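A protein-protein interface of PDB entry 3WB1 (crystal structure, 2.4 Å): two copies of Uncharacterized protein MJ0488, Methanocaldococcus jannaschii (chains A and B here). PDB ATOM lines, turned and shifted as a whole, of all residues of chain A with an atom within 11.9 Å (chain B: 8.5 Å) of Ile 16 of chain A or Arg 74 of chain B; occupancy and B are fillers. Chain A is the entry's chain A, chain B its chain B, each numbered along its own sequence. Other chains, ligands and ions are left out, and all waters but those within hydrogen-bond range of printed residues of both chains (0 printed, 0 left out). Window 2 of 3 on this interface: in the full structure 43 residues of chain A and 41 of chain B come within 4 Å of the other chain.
The backbone carbonyl oxygen (O) of Ser 15 of chain A lies within hydrogen-bond range of the guanidinium group (NH1) of Arg 74 of chain B, 2.5 Å away.
The backbone NH (N) of Asn 18 of chain A sits close to the guanidinium group (NH1) of Arg 74 of chain B (3.3 Å).
The backbone carbonyl oxygen (O) of Ile 16 of chain A sits at hydrogen-bond distance from the guanidinium group (NH1) of Arg 74 of chain B, 2.5 Å away.
The guanidinium group of Arg 104 of chain B is in hydrogen-bond range of the backbone carbonyl oxygen of Asp 77 of chain B (3.1 Å).
The side-chain carboxylate (OD2) of Asp 72 of chain B is in salt-bridge range of the guanidinium group (NE) of Arg 74 of chain B (3.0 Å).
The backbone carbonyl oxygen (O) of Ala 11 of chain A sits at hydrogen-bond distance from the side-chain hydroxyl (OG) of Ser 15 of chain A (3.2 Å).
The guanidinium group (NH1) of Arg 20 of chain A is in salt-bridge range of the side-chain carboxylate (OE2) of Glu 27 of chain A.
NH2 of Arg 20 of chain A is in salt-bridge range of OD1 of Asp 23 of chain A (3.2 Å).
The backbone carbonyl oxygen of Ile 13 of chain A lies close to the side-chain amide oxygen of Asn 17 of chain A.
O of Asp 77 of chain B touches CE1 of Phe 12 of chain A (3.4 Å).
Phe 12 of chain A touches Leu 78 of chain B (CZ to O, 3.4 Å).
Ser 15 of chain A touches Asp 77 of chain B (OG to CB, 3.7 Å).
Ser 15 of chain A touches Arg 104 of chain B (OG to NH1, 3.99 Å).
Arg 74 of chain B touches Asn 17 of chain A.
Arg 20 of chain A touches Arg 104 of chain B (NE to NH1, 3.9 Å).
Of the printed residues of chain B, Phe 12 of chain A touches Asp 77 (3.4 Å) and Leu 78 (3.4 Å).
Printed residues of chain B within 4 Å of Ser 15 of chain A: Arg 74 (2.5 Å), Asp 77 (3.7 Å) and Arg 104 (3.99 Å).
Ile 16 of chain A touches just one residue of chain B: Arg 74.
Of the printed residues of chain B, Asn 18 of chain A touches Arg 74 (3.3 Å).
Printed residues of chain B within 4 Å of Arg 20 of chain A: Arg 104 (3.9 Å).
Gly 22 of chain A touches none of the printed residues of chain B.
No residue of chain A comes within 4 Å of Asp 72 of chain B.
No residue of chain A comes within 4 Å of Thr 73 of chain B.
Of chain A, only Ser 15 (2.5 Å), Ile 16 (2.5 Å), Asn 17 (3.8 Å) and Asn 18 (3.3 Å) come within 4 Å of Arg 74 of chain B.
No residue of chain A comes within 4 Å of Phe 75 of chain B.
Asp 77 of chain B touches just these residues of chain A: Phe 12 (3.4 Å) and Ser 15 (3.7 Å).
Of the printed residues of chain A, Leu 78 of chain B touches Phe 12.
The nearest residue of chain B that does not touch Ile 16 of chain A is Leu 78 of chain B (4.1 Å).
The nearest residue of chain A that does not touch Arg 74 of chain B is Glu 14 of chain A (5.3 Å).
The nearest printed residue of chain B that does not touch Asn 17 of chain A is Phe 75 of chain B (6.8 Å).
Of the 18 printed residues of chain A, 6 touch a printed residue of chain B.
Hydrophobic or aromatic side chains of chain A that line the printed part of chain B: Phe 12.
Of the 18 printed residues of chain B, 4 touch a printed residue of chain A.
Hydrophobic or aromatic side chains of chain B within 4 Å of the printed part of chain A: Leu 78.
Among the printed residues, 9 pairs touch across the chains.
No position is printed for both chains.
Of the 9 pairs that touch across the chains among the printed residues, none has its exchanged pair printed and touching as well.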
ATOM      1  N   ILE A   7       7.715 -12.812 -35.288  1.00  0.00           N
ATOM      2  CA  ILE A   7       8.130 -12.814 -33.895  1.00  0.00           C
ATOM      3  C   ILE A   7       7.365 -11.735 -33.138  1.00  0.00           C
ATOM      4  O   ILE A   7       6.900 -11.961 -32.019  1.00  0.00           O
ATOM      5  CB  ILE A   7       9.662 -12.626 -33.773  1.00  0.00           C
ATOM      6  CG1 ILE A   7      10.378 -13.891 -34.262  1.00  0.00           C
ATOM      7  CG2 ILE A   7      10.061 -12.330 -32.351  1.00  0.00           C
ATOM      8  CD1 ILE A   7      11.896 -13.813 -34.250  1.00  0.00           C
ATOM      9  N   ILE A   8       7.185 -10.582 -33.775  1.00  0.00           N
ATOM     10  CA  ILE A   8       6.451  -9.476 -33.162  1.00  0.00           C
ATOM     11  C   ILE A   8       4.945  -9.777 -33.061  1.00  0.00           C
ATOM     12  O   ILE A   8       4.301  -9.415 -32.071  1.00  0.00           O
ATOM     13  CB  ILE A   8       6.678  -8.161 -33.946  1.00  0.00           C
ATOM     14  CG1 ILE A   8       8.160  -7.782 -33.930  1.00  0.00           C
ATOM     15  CG2 ILE A   8       5.833  -7.018 -33.384  1.00  0.00           C
ATOM     16  CD1 ILE A   8       8.462  -6.501 -34.665  1.00  0.00           C
ATOM     17  N   LYS A   9       4.396 -10.453 -34.071  1.00  0.00           N
ATOM     18  CA  LYS A   9       2.986 -10.856 -34.069  1.00  0.00           C
ATOM     19  C   LYS A   9       2.626 -11.661 -32.814  1.00  0.00           C
ATOM     20  O   LYS A   9       1.642 -11.356 -32.133  1.00  0.00           O
ATOM     21  CB  LYS A   9       2.657 -11.665 -35.333  1.00  0.00           C
ATOM     22  CG  LYS A   9       1.155 -11.769 -35.649  1.00  0.00           C
ATOM     23  CD  LYS A   9       0.825 -13.012 -36.477  1.00  0.00           C
ATOM     24  CE  LYS A   9      -0.431 -12.818 -37.330  1.00  0.00           C
ATOM     25  NZ  LYS A   9      -0.174 -12.038 -38.581  1.00  0.00           N
ATOM     26  N   LYS A  10       3.434 -12.672 -32.500  1.00  0.00           N
ATOM     27  CA  LYS A  10       3.211 -13.496 -31.312  1.00  0.00           C
ATOM     28  C   LYS A  10       3.248 -12.669 -30.028  1.00  0.00           C
ATOM     29  O   LYS A  10       2.489 -12.924 -29.092  1.00  0.00           O
ATOM     30  CB  LYS A  10       4.257 -14.596 -31.210  1.00  0.00           C
ATOM     31  CG  LYS A  10       4.297 -15.565 -32.363  1.00  0.00           C
ATOM     32  CD  LYS A  10       5.176 -16.738 -31.971  1.00  0.00           C
ATOM     33  CE  LYS A  10       6.641 -16.328 -31.950  1.00  0.00           C
ATOM     34  NZ  LYS A  10       7.550 -17.466 -31.618  1.00  0.00           N
ATOM     35  N   ALA A  11       4.165 -11.709 -29.969  1.00  0.00           N
ATOM     36  CA  ALA A  11       4.269 -10.845 -28.800  1.00  0.00           C
ATOM     37  C   ALA A  11       3.028  -9.965 -28.666  1.00  0.00           C
ATOM     38  O   ALA A  11       2.480  -9.822 -27.574  1.00  0.00           O
ATOM     39  CB  ALA A  11       5.531  -9.988 -28.877  1.00  0.00           C
ATOM     40  N   PHE A  12       2.563  -9.414 -29.784  1.00  0.00           N
ATOM     41  CA  PHE A  12       1.388  -8.550 -29.767  1.00  0.00           C
ATOM     42  C   PHE A  12       0.162  -9.331 -29.319  1.00  0.00           C
ATOM     43  O   PHE A  12      -0.690  -8.799 -28.605  1.00  0.00           O
ATOM     44  CB  PHE A  12       1.125  -7.937 -31.147  1.00  0.00           C
ATOM     45  CG  PHE A  12       2.010  -6.766 -31.492  1.00  0.00           C
ATOM     46  CD1 PHE A  12       3.085  -6.410 -30.689  1.00  0.00           C
ATOM     47  CD2 PHE A  12       1.724  -5.982 -32.606  1.00  0.00           C
ATOM     48  CE1 PHE A  12       3.888  -5.318 -31.015  1.00  0.00           C
ATOM     49  CE2 PHE A  12       2.513  -4.886 -32.940  1.00  0.00           C
ATOM     50  CZ  PHE A  12       3.598  -4.552 -32.140  1.00  0.00           C
ATOM     51  N   ILE A  13       0.075 -10.592 -29.739  1.00  0.00           N
ATOM     52  CA  ILE A  13      -1.039 -11.456 -29.361  1.00  0.00           C
ATOM     53  C   ILE A  13      -0.989 -11.793 -27.868  1.00  0.00           C
ATOM     54  O   ILE A  13      -2.020 -11.826 -27.191  1.00  0.00           O
ATOM     55  CB  ILE A  13      -1.045 -12.762 -30.196  1.00  0.00           C
ATOM     56  CG1 ILE A  13      -1.330 -12.462 -31.669  1.00  0.00           C
ATOM     57  CG2 ILE A  13      -2.081 -13.755 -29.675  1.00  0.00           C
ATOM     58  CD1 ILE A  13      -1.293 -13.695 -32.550  1.00  0.00           C
ATOM     59  N   GLU A  14       0.215 -12.036 -27.359  1.00  0.00           N
ATOM     60  CA  GLU A  14       0.403 -12.310 -25.937  1.00  0.00           C
ATOM     61  C   GLU A  14      -0.067 -11.135 -25.094  1.00  0.00           C
ATOM     62  O   GLU A  14      -0.650 -11.323 -24.027  1.00  0.00           O
ATOM     63  CB  GLU A  14       1.871 -12.599 -25.621  1.00  0.00           C
ATOM     64  CG  GLU A  14       2.375 -13.960 -26.067  1.00  0.00           C
ATOM     65  CD  GLU A  14       3.832 -14.164 -25.711  1.00  0.00           C
ATOM     66  OE1 GLU A  14       4.568 -13.158 -25.617  1.00  0.00           O
ATOM     67  OE2 GLU A  14       4.244 -15.325 -25.528  1.00  0.00           O
ATOM     68  N   SER A  15       0.196  -9.926 -25.585  1.00  0.00           N
ATOM     69  CA  SER A  15      -0.174  -8.701 -24.884  1.00  0.00           C
ATOM     70  C   SER A  15      -1.686  -8.506 -24.915  1.00  0.00           C
ATOM     71  O   SER A  15      -2.287  -8.076 -23.932  1.00  0.00           O
ATOM     72  CB  SER A  15       0.527  -7.489 -25.507  1.00  0.00           C
ATOM     73  OG  SER A  15       1.937  -7.564 -25.362  1.00  0.00           O
ATOM     74  N   ILE A  16      -2.288  -8.807 -26.060  1.00  0.00           N
ATOM     75  CA  ILE A  16      -3.738  -8.725 -26.222  1.00  0.00           C
ATOM     76  C   ILE A  16      -4.444  -9.668 -25.248  1.00  0.00           C
ATOM     77  O   ILE A  16      -5.432  -9.296 -24.605  1.00  0.00           O
ATOM     78  CB  ILE A  16      -4.176  -9.057 -27.671  1.00  0.00           C
ATOM     79  CG1 ILE A  16      -3.814  -7.910 -28.624  1.00  0.00           C
ATOM     80  CG2 ILE A  16      -5.675  -9.331 -27.739  1.00  0.00           C
ATOM     81  CD1 ILE A  16      -4.190  -8.170 -30.083  1.00  0.00           C
ATOM     82  N   ASN A  17      -3.914 -10.877 -25.106  1.00  0.00           N
ATOM     83  CA  ASN A  17      -4.559 -11.876 -24.269  1.00  0.00           C
ATOM     84  C   ASN A  17      -3.983 -11.912 -22.850  1.00  0.00           C
ATOM     85  O   ASN A  17      -4.186 -12.880 -22.112  1.00  0.00           O
ATOM     86  CB  ASN A  17      -4.447 -13.254 -24.916  1.00  0.00           C
ATOM     87  CG  ASN A  17      -5.143 -13.323 -26.261  1.00  0.00           C
ATOM     88  OD1 ASN A  17      -4.553 -13.759 -27.251  1.00  0.00           O
ATOM     89  ND2 ASN A  17      -6.394 -12.870 -26.312  1.00  0.00           N
ATOM     90  N   ASN A  18      -3.251 -10.859 -22.491  1.00  0.00           N
ATOM     91  CA  ASN A  18      -2.797 -10.631 -21.120  1.00  0.00           C
ATOM     92  C   ASN A  18      -1.975 -11.774 -20.531  1.00  0.00           C
ATOM     93  O   ASN A  18      -2.184 -12.162 -19.383  1.00  0.00           O
ATOM     94  CB  ASN A  18      -4.011 -10.369 -20.223  1.00  0.00           C
ATOM     95  CG  ASN A  18      -3.668  -9.571 -18.983  1.00  0.00           C
ATOM     96  OD1 ASN A  18      -2.557  -9.056 -18.847  1.00  0.00           O
ATOM     97  ND2 ASN A  18      -4.615  -9.494 -18.053  1.00  0.00           N
ATOM     98  N   ILE A  19      -1.054 -12.323 -21.318  1.00  0.00           N
ATOM     99  CA  ILE A  19      -0.111 -13.324 -20.815  1.00  0.00           C
ATOM    100  C   ILE A  19       1.337 -12.900 -21.028  1.00  0.00           C
ATOM    101  O   ILE A  19       2.257 -13.680 -20.784  1.00  0.00           O
ATOM    102  CB  ILE A  19      -0.332 -14.715 -21.451  1.00  0.00           C
ATOM    103  CG1 ILE A  19      -0.333 -14.618 -22.979  1.00  0.00           C
ATOM    104  CG2 ILE A  19      -1.630 -15.335 -20.945  1.00  0.00           C
ATOM    105  CD1 ILE A  19      -0.532 -15.954 -23.672  1.00  0.00           C
ATOM    106  N   ARG A  20       1.531 -11.664 -21.480  1.00  0.00           N
ATOM    107  CA  ARG A  20       2.871 -11.153 -21.751  1.00  0.00           C
ATOM    108  C   ARG A  20       3.680 -10.998 -20.456  1.00  0.00           C
ATOM    109  O   ARG A  20       3.334 -10.216 -19.569  1.00  0.00           O
ATOM    110  CB  ARG A  20       2.777  -9.813 -22.494  1.00  0.00           C
ATOM    111  CG  ARG A  20       4.109  -9.164 -22.859  1.00  0.00           C
ATOM    112  CD  ARG A  20       4.800  -9.852 -24.029  1.00  0.00           C
ATOM    113  NE  ARG A  20       6.072  -9.209 -24.368  1.00  0.00           N
ATOM    114  CZ  ARG A  20       6.940  -9.684 -25.259  1.00  0.00           C
ATOM    115  NH1 ARG A  20       6.683 -10.820 -25.894  1.00  0.00           N
ATOM    116  NH2 ARG A  20       8.068  -9.031 -25.508  1.00  0.00           N
ATOM    117  N   ARG A  21       4.766 -11.760 -20.370  1.00  0.00           N
ATOM    118  CA  ARG A  21       5.685 -11.726 -19.234  1.00  0.00           C
ATOM    119  C   ARG A  21       7.118 -11.502 -19.701  1.00  0.00           C
ATOM    120  O   ARG A  21       7.921 -12.437 -19.758  1.00  0.00           O
ATOM    121  CB  ARG A  21       5.613 -13.027 -18.426  1.00  0.00           C
ATOM    122  CG  ARG A  21       6.537 -13.042 -17.203  1.00  0.00           C
ATOM    123  CD  ARG A  21       6.479 -14.353 -16.428  1.00  0.00           C
ATOM    124  NE  ARG A  21       7.479 -14.372 -15.361  1.00  0.00           N
ATOM    125  CZ  ARG A  21       7.486 -15.226 -14.342  1.00  0.00           C
ATOM    126  NH1 ARG A  21       6.537 -16.145 -14.230  1.00  0.00           N
ATOM    127  NH2 ARG A  21       8.448 -15.161 -13.431  1.00  0.00           N
ATOM    128  N   GLY A  22       7.431 -10.266 -20.065  1.00  0.00           N
ATOM    129  CA  GLY A  22       8.783  -9.926 -20.458  1.00  0.00           C
ATOM    130  C   GLY A  22       9.173 -10.409 -21.843  1.00  0.00           C
ATOM    131  O   GLY A  22       8.411 -11.112 -22.515  1.00  0.00           O
ATOM    132  N   ASP A  23      10.378 -10.036 -22.260  1.00  0.00           N
ATOM    133  CA  ASP A  23      10.896 -10.390 -23.575  1.00  0.00           C
ATOM    134  C   ASP A  23      11.212 -11.878 -23.683  1.00  0.00           C
ATOM    135  O   ASP A  23      11.473 -12.542 -22.680  1.00  0.00           O
ATOM    136  CB  ASP A  23      12.134  -9.555 -23.889  1.00  0.00           C
ATOM    137  CG  ASP A  23      11.835  -8.063 -23.946  1.00  0.00           C
ATOM    138  OD1 ASP A  23      10.654  -7.696 -24.157  1.00  0.00           O
ATOM    139  OD2 ASP A  23      12.778  -7.258 -23.780  1.00  0.00           O
ATOM    140  N   GLU A  27      13.143 -13.346 -29.463  1.00  0.00           N
ATOM    141  CA  GLU A  27      13.119 -11.917 -29.791  1.00  0.00           C
ATOM    142  C   GLU A  27      14.519 -11.315 -29.726  1.00  0.00           C
ATOM    143  O   GLU A  27      14.907 -10.509 -30.570  1.00  0.00           O
ATOM    144  CB  GLU A  27      12.171 -11.160 -28.848  1.00  0.00           C
ATOM    145  CG  GLU A  27      10.713 -11.638 -28.949  1.00  0.00           C
ATOM    146  CD  GLU A  27       9.863 -11.272 -27.747  1.00  0.00           C
ATOM    147  OE1 GLU A  27      10.409 -10.721 -26.767  1.00  0.00           O
ATOM    148  OE2 GLU A  27       8.647 -11.569 -27.773  1.00  0.00           O
ATOM    149  N   ALA B  44       2.084   6.113 -14.878  1.00  0.00           N
ATOM    150  CA  ALA B  44       1.339   5.335 -15.862  1.00  0.00           C
ATOM    151  C   ALA B  44       1.611   3.847 -15.719  1.00  0.00           C
ATOM    152  O   ALA B  44       2.309   3.250 -16.544  1.00  0.00           O
ATOM    153  CB  ALA B  44       1.667   5.797 -17.269  1.00  0.00           C
ATOM    154  N   THR B  45       1.060   3.248 -14.671  1.00  0.00           N
ATOM    155  CA  THR B  45       1.200   1.817 -14.465  1.00  0.00           C
ATOM    156  C   THR B  45      -0.027   1.308 -13.735  1.00  0.00           C
ATOM    157  O   THR B  45      -0.819   2.099 -13.224  1.00  0.00           O
ATOM    158  CB  THR B  45       2.466   1.474 -13.654  1.00  0.00           C
ATOM    159  OG1 THR B  45       2.643   0.053 -13.595  1.00  0.00           O
ATOM    160  CG2 THR B  45       2.355   2.027 -12.240  1.00  0.00           C
ATOM    161  N   ASN B  46      -0.183  -0.011 -13.696  1.00  0.00           N
ATOM    162  CA  ASN B  46      -1.228  -0.639 -12.895  1.00  0.00           C
ATOM    163  C   ASN B  46      -0.623  -1.561 -11.849  1.00  0.00           C
ATOM    164  O   ASN B  46      -1.324  -2.082 -10.977  1.00  0.00           O
ATOM    165  CB  ASN B  46      -2.199  -1.417 -13.778  1.00  0.00           C
ATOM    166  CG  ASN B  46      -2.789  -0.569 -14.881  1.00  0.00           C
ATOM    167  OD1 ASN B  46      -2.339  -0.618 -16.029  1.00  0.00           O
ATOM    168  ND2 ASN B  46      -3.795   0.227 -14.537  1.00  0.00           N
ATOM    169  N   ILE B  71      -6.391   2.869 -15.496  1.00  0.00           N
ATOM    170  CA  ILE B  71      -6.615   1.967 -16.625  1.00  0.00           C
ATOM    171  C   ILE B  71      -5.400   1.110 -16.971  1.00  0.00           C
ATOM    172  O   ILE B  71      -4.268   1.439 -16.609  1.00  0.00           O
ATOM    173  CB  ILE B  71      -7.014   2.760 -17.883  1.00  0.00           C
ATOM    174  CG1 ILE B  71      -5.822   3.569 -18.386  1.00  0.00           C
ATOM    175  CG2 ILE B  71      -8.179   3.691 -17.581  1.00  0.00           C
ATOM    176  CD1 ILE B  71      -6.091   4.268 -19.687  1.00  0.00           C
ATOM    177  N   ASP B  72      -5.657   0.027 -17.705  1.00  0.00           N
ATOM    178  CA  ASP B  72      -4.630  -0.942 -18.079  1.00  0.00           C
ATOM    179  C   ASP B  72      -3.856  -0.464 -19.297  1.00  0.00           C
ATOM    180  O   ASP B  72      -4.430  -0.240 -20.358  1.00  0.00           O
ATOM    181  CB  ASP B  72      -5.277  -2.307 -18.352  1.00  0.00           C
ATOM    182  CG  ASP B  72      -4.267  -3.438 -18.440  1.00  0.00           C
ATOM    183  OD1 ASP B  72      -3.062  -3.203 -18.197  1.00  0.00           O
ATOM    184  OD2 ASP B  72      -4.693  -4.576 -18.739  1.00  0.00           O
ATOM    185  N   THR B  73      -2.548  -0.308 -19.139  1.00  0.00           N
ATOM    186  CA  THR B  73      -1.720   0.229 -20.210  1.00  0.00           C
ATOM    187  C   THR B  73      -0.949  -0.853 -20.968  1.00  0.00           C
ATOM    188  O   THR B  73       0.021  -0.557 -21.670  1.00  0.00           O
ATOM    189  CB  THR B  73      -0.726   1.263 -19.656  1.00  0.00           C
ATOM    190  OG1 THR B  73      -0.265   0.838 -18.365  1.00  0.00           O
ATOM    191  CG2 THR B  73      -1.403   2.618 -19.516  1.00  0.00           C
ATOM    192  N   ARG B  74      -1.390  -2.101 -20.834  1.00  0.00           N
ATOM    193  CA  ARG B  74      -0.735  -3.225 -21.499  1.00  0.00           C
ATOM    194  C   ARG B  74      -0.932  -3.157 -23.014  1.00  0.00           C
ATOM    195  O   ARG B  74      -0.180  -3.751 -23.793  1.00  0.00           O
ATOM    196  CB  ARG B  74      -1.260  -4.547 -20.925  1.00  0.00           C
ATOM    197  CG  ARG B  74      -2.723  -4.872 -21.253  1.00  0.00           C
ATOM    198  CD  ARG B  74      -3.038  -6.342 -20.949  1.00  0.00           C
ATOM    199  NE  ARG B  74      -4.476  -6.620 -20.913  1.00  0.00           N
ATOM    200  CZ  ARG B  74      -5.137  -7.319 -21.833  1.00  0.00           C
ATOM    201  NH1 ARG B  74      -4.489  -7.823 -22.873  1.00  0.00           N
ATOM    202  NH2 ARG B  74      -6.446  -7.526 -21.708  1.00  0.00           N
ATOM    203  N   PHE B  75      -1.939  -2.399 -23.418  1.00  0.00           N
ATOM    204  CA  PHE B  75      -2.268  -2.240 -24.820  1.00  0.00           C
ATOM    205  C   PHE B  75      -1.289  -1.296 -25.504  1.00  0.00           C
ATOM    206  O   PHE B  75      -1.212  -1.252 -26.736  1.00  0.00           O
ATOM    207  CB  PHE B  75      -3.694  -1.730 -24.938  1.00  0.00           C
ATOM    208  CG  PHE B  75      -4.657  -2.513 -24.106  1.00  0.00           C
ATOM    209  CD1 PHE B  75      -5.045  -3.782 -24.494  1.00  0.00           C
ATOM    210  CD2 PHE B  75      -5.131  -2.003 -22.906  1.00  0.00           C
ATOM    211  CE1 PHE B  75      -5.918  -4.517 -23.724  1.00  0.00           C
ATOM    212  CE2 PHE B  75      -6.001  -2.734 -22.127  1.00  0.00           C
ATOM    213  CZ  PHE B  75      -6.396  -3.994 -22.536  1.00  0.00           C
ATOM    214  N   ALA B  76      -0.536  -0.549 -24.700  1.00  0.00           N
ATOM    215  CA  ALA B  76       0.521   0.302 -25.228  1.00  0.00           C
ATOM    216  C   ALA B  76       1.605  -0.548 -25.864  1.00  0.00           C
ATOM    217  O   ALA B  76       2.372  -0.078 -26.705  1.00  0.00           O
ATOM    218  CB  ALA B  76       1.107   1.177 -24.127  1.00  0.00           C
ATOM    219  N   ASP B  77       1.650  -1.814 -25.469  1.00  0.00           N
ATOM    220  CA  ASP B  77       2.659  -2.737 -25.969  1.00  0.00           C
ATOM    221  C   ASP B  77       2.411  -3.162 -27.415  1.00  0.00           C
ATOM    222  O   ASP B  77       3.123  -4.019 -27.941  1.00  0.00           O
ATOM    223  CB  ASP B  77       2.735  -3.964 -25.063  1.00  0.00           C
ATOM    224  CG  ASP B  77       3.253  -3.626 -23.680  1.00  0.00           C
ATOM    225  OD1 ASP B  77       3.940  -2.594 -23.543  1.00  0.00           O
ATOM    226  OD2 ASP B  77       2.977  -4.392 -22.734  1.00  0.00           O
ATOM    227  N   LEU B  78       1.387  -2.591 -28.044  1.00  0.00           N
ATOM    228  CA  LEU B  78       1.135  -2.832 -29.458  1.00  0.00           C
ATOM    229  C   LEU B  78       1.769  -1.715 -30.277  1.00  0.00           C
ATOM    230  O   LEU B  78       1.777  -1.758 -31.508  1.00  0.00           O
ATOM    231  CB  LEU B  78      -0.369  -2.917 -29.760  1.00  0.00           C
ATOM    232  CG  LEU B  78      -1.218  -3.985 -29.051  1.00  0.00           C
ATOM    233  CD1 LEU B  78      -2.695  -3.854 -29.432  1.00  0.00           C
ATOM    234  CD2 LEU B  78      -0.718  -5.394 -29.342  1.00  0.00           C
ATOM    235  N   THR B  79       2.286  -0.695 -29.597  1.00  0.00           N
ATOM    236  CA  THR B  79       2.832   0.452 -30.309  1.00  0.00           C
ATOM    237  C   THR B  79       4.340   0.333 -30.462  1.00  0.00           C
ATOM    238  O   THR B  79       4.977  -0.546 -29.861  1.00  0.00           O
ATOM    239  CB  THR B  79       2.510   1.790 -29.588  1.00  0.00           C
ATOM    240  OG1 THR B  79       3.272   1.901 -28.374  1.00  0.00           O
ATOM    241  CG2 THR B  79       1.009   1.899 -29.303  1.00  0.00           C
ATOM    242  N   PRO B  82       6.149   1.560 -26.439  1.00  0.00           N
ATOM    243  CA  PRO B  82       5.110   1.388 -25.414  1.00  0.00           C
ATOM    244  C   PRO B  82       5.256   2.292 -24.202  1.00  0.00           C
ATOM    245  O   PRO B  82       4.252   2.821 -23.733  1.00  0.00           O
ATOM    246  CB  PRO B  82       5.273  -0.075 -25.001  1.00  0.00           C
ATOM    247  CG  PRO B  82       5.872  -0.731 -26.201  1.00  0.00           C
ATOM    248  CD  PRO B  82       6.815   0.287 -26.761  1.00  0.00           C
ATOM    249  N   THR B  85       4.062   5.646 -25.006  1.00  0.00           N
ATOM    250  CA  THR B  85       2.621   5.589 -25.239  1.00  0.00           C
ATOM    251  C   THR B  85       1.848   5.675 -23.930  1.00  0.00           C
ATOM    252  O   THR B  85       0.855   6.405 -23.827  1.00  0.00           O
ATOM    253  CB  THR B  85       2.228   4.296 -25.988  1.00  0.00           C
ATOM    254  OG1 THR B  85       2.852   4.281 -27.281  1.00  0.00           O
ATOM    255  CG2 THR B  85       0.724   4.211 -26.163  1.00  0.00           C
ATOM    256  N   LYS B  86       2.327   4.937 -22.932  1.00  0.00           N
ATOM    257  CA  LYS B  86       1.741   4.938 -21.595  1.00  0.00           C
ATOM    258  C   LYS B  86       1.736   6.328 -20.969  1.00  0.00           C
ATOM    259  O   LYS B  86       0.756   6.735 -20.331  1.00  0.00           O
ATOM    260  CB  LYS B  86       2.506   3.980 -20.687  1.00  0.00           C
ATOM    261  CG  LYS B  86       2.412   2.518 -21.103  1.00  0.00           C
ATOM    262  CD  LYS B  86       3.213   1.647 -20.139  1.00  0.00           C
ATOM    263  CE  LYS B  86       2.979   0.169 -20.380  1.00  0.00           C
ATOM    264  NZ  LYS B  86       3.799  -0.648 -19.437  1.00  0.00           N
ATOM    265  N   ILE B  89      -0.798   8.394 -22.776  1.00  0.00           N
ATOM    266  CA  ILE B  89      -2.129   7.991 -22.329  1.00  0.00           C
ATOM    267  C   ILE B  89      -2.466   8.693 -21.004  1.00  0.00           C
ATOM    268  O   ILE B  89      -3.554   9.257 -20.838  1.00  0.00           O
ATOM    269  CB  ILE B  89      -2.235   6.460 -22.162  1.00  0.00           C
ATOM    270  CG1 ILE B  89      -2.346   5.778 -23.533  1.00  0.00           C
ATOM    271  CG2 ILE B  89      -3.427   6.095 -21.280  1.00  0.00           C
ATOM    272  CD1 ILE B  89      -2.249   4.254 -23.488  1.00  0.00           C
ATOM    273  N   ARG B 102       6.701   3.597 -17.238  1.00  0.00           N
ATOM    274  CA  ARG B 102       7.687   2.541 -17.415  1.00  0.00           C
ATOM    275  C   ARG B 102       7.111   1.419 -18.278  1.00  0.00           C
ATOM    276  O   ARG B 102       6.002   0.934 -18.019  1.00  0.00           O
ATOM    277  CB  ARG B 102       8.129   1.979 -16.062  1.00  0.00           C
ATOM    278  CG  ARG B 102       9.455   1.244 -16.132  1.00  0.00           C
ATOM    279  CD  ARG B 102       9.431  -0.082 -15.405  1.00  0.00           C
ATOM    280  NE  ARG B 102      10.711  -0.773 -15.558  1.00  0.00           N
ATOM    281  CZ  ARG B 102      10.833  -2.062 -15.857  1.00  0.00           C
ATOM    282  NH1 ARG B 102       9.754  -2.812 -16.019  1.00  0.00           N
ATOM    283  NH2 ARG B 102      12.034  -2.602 -15.988  1.00  0.00           N
ATOM    284  N   ARG B 104       8.138  -1.147 -22.219  1.00  0.00           N
ATOM    285  CA  ARG B 104       9.080  -1.580 -23.243  1.00  0.00           C
ATOM    286  C   ARG B 104       9.666  -0.358 -23.954  1.00  0.00           C
ATOM    287  O   ARG B 104       8.983   0.660 -24.116  1.00  0.00           O
ATOM    288  CB  ARG B 104       8.392  -2.495 -24.268  1.00  0.00           C
ATOM    289  CG  ARG B 104       9.359  -3.259 -25.148  1.00  0.00           C
ATOM    290  CD  ARG B 104       8.662  -4.037 -26.248  1.00  0.00           C
ATOM    291  NE  ARG B 104       7.532  -4.852 -25.814  1.00  0.00           N
ATOM    292  CZ  ARG B 104       6.368  -4.909 -26.457  1.00  0.00           C
ATOM    293  NH1 ARG B 104       5.396  -5.690 -26.007  1.00  0.00           N
ATOM    294  NH2 ARG B 104       6.168  -4.174 -27.544  1.00  0.00           N
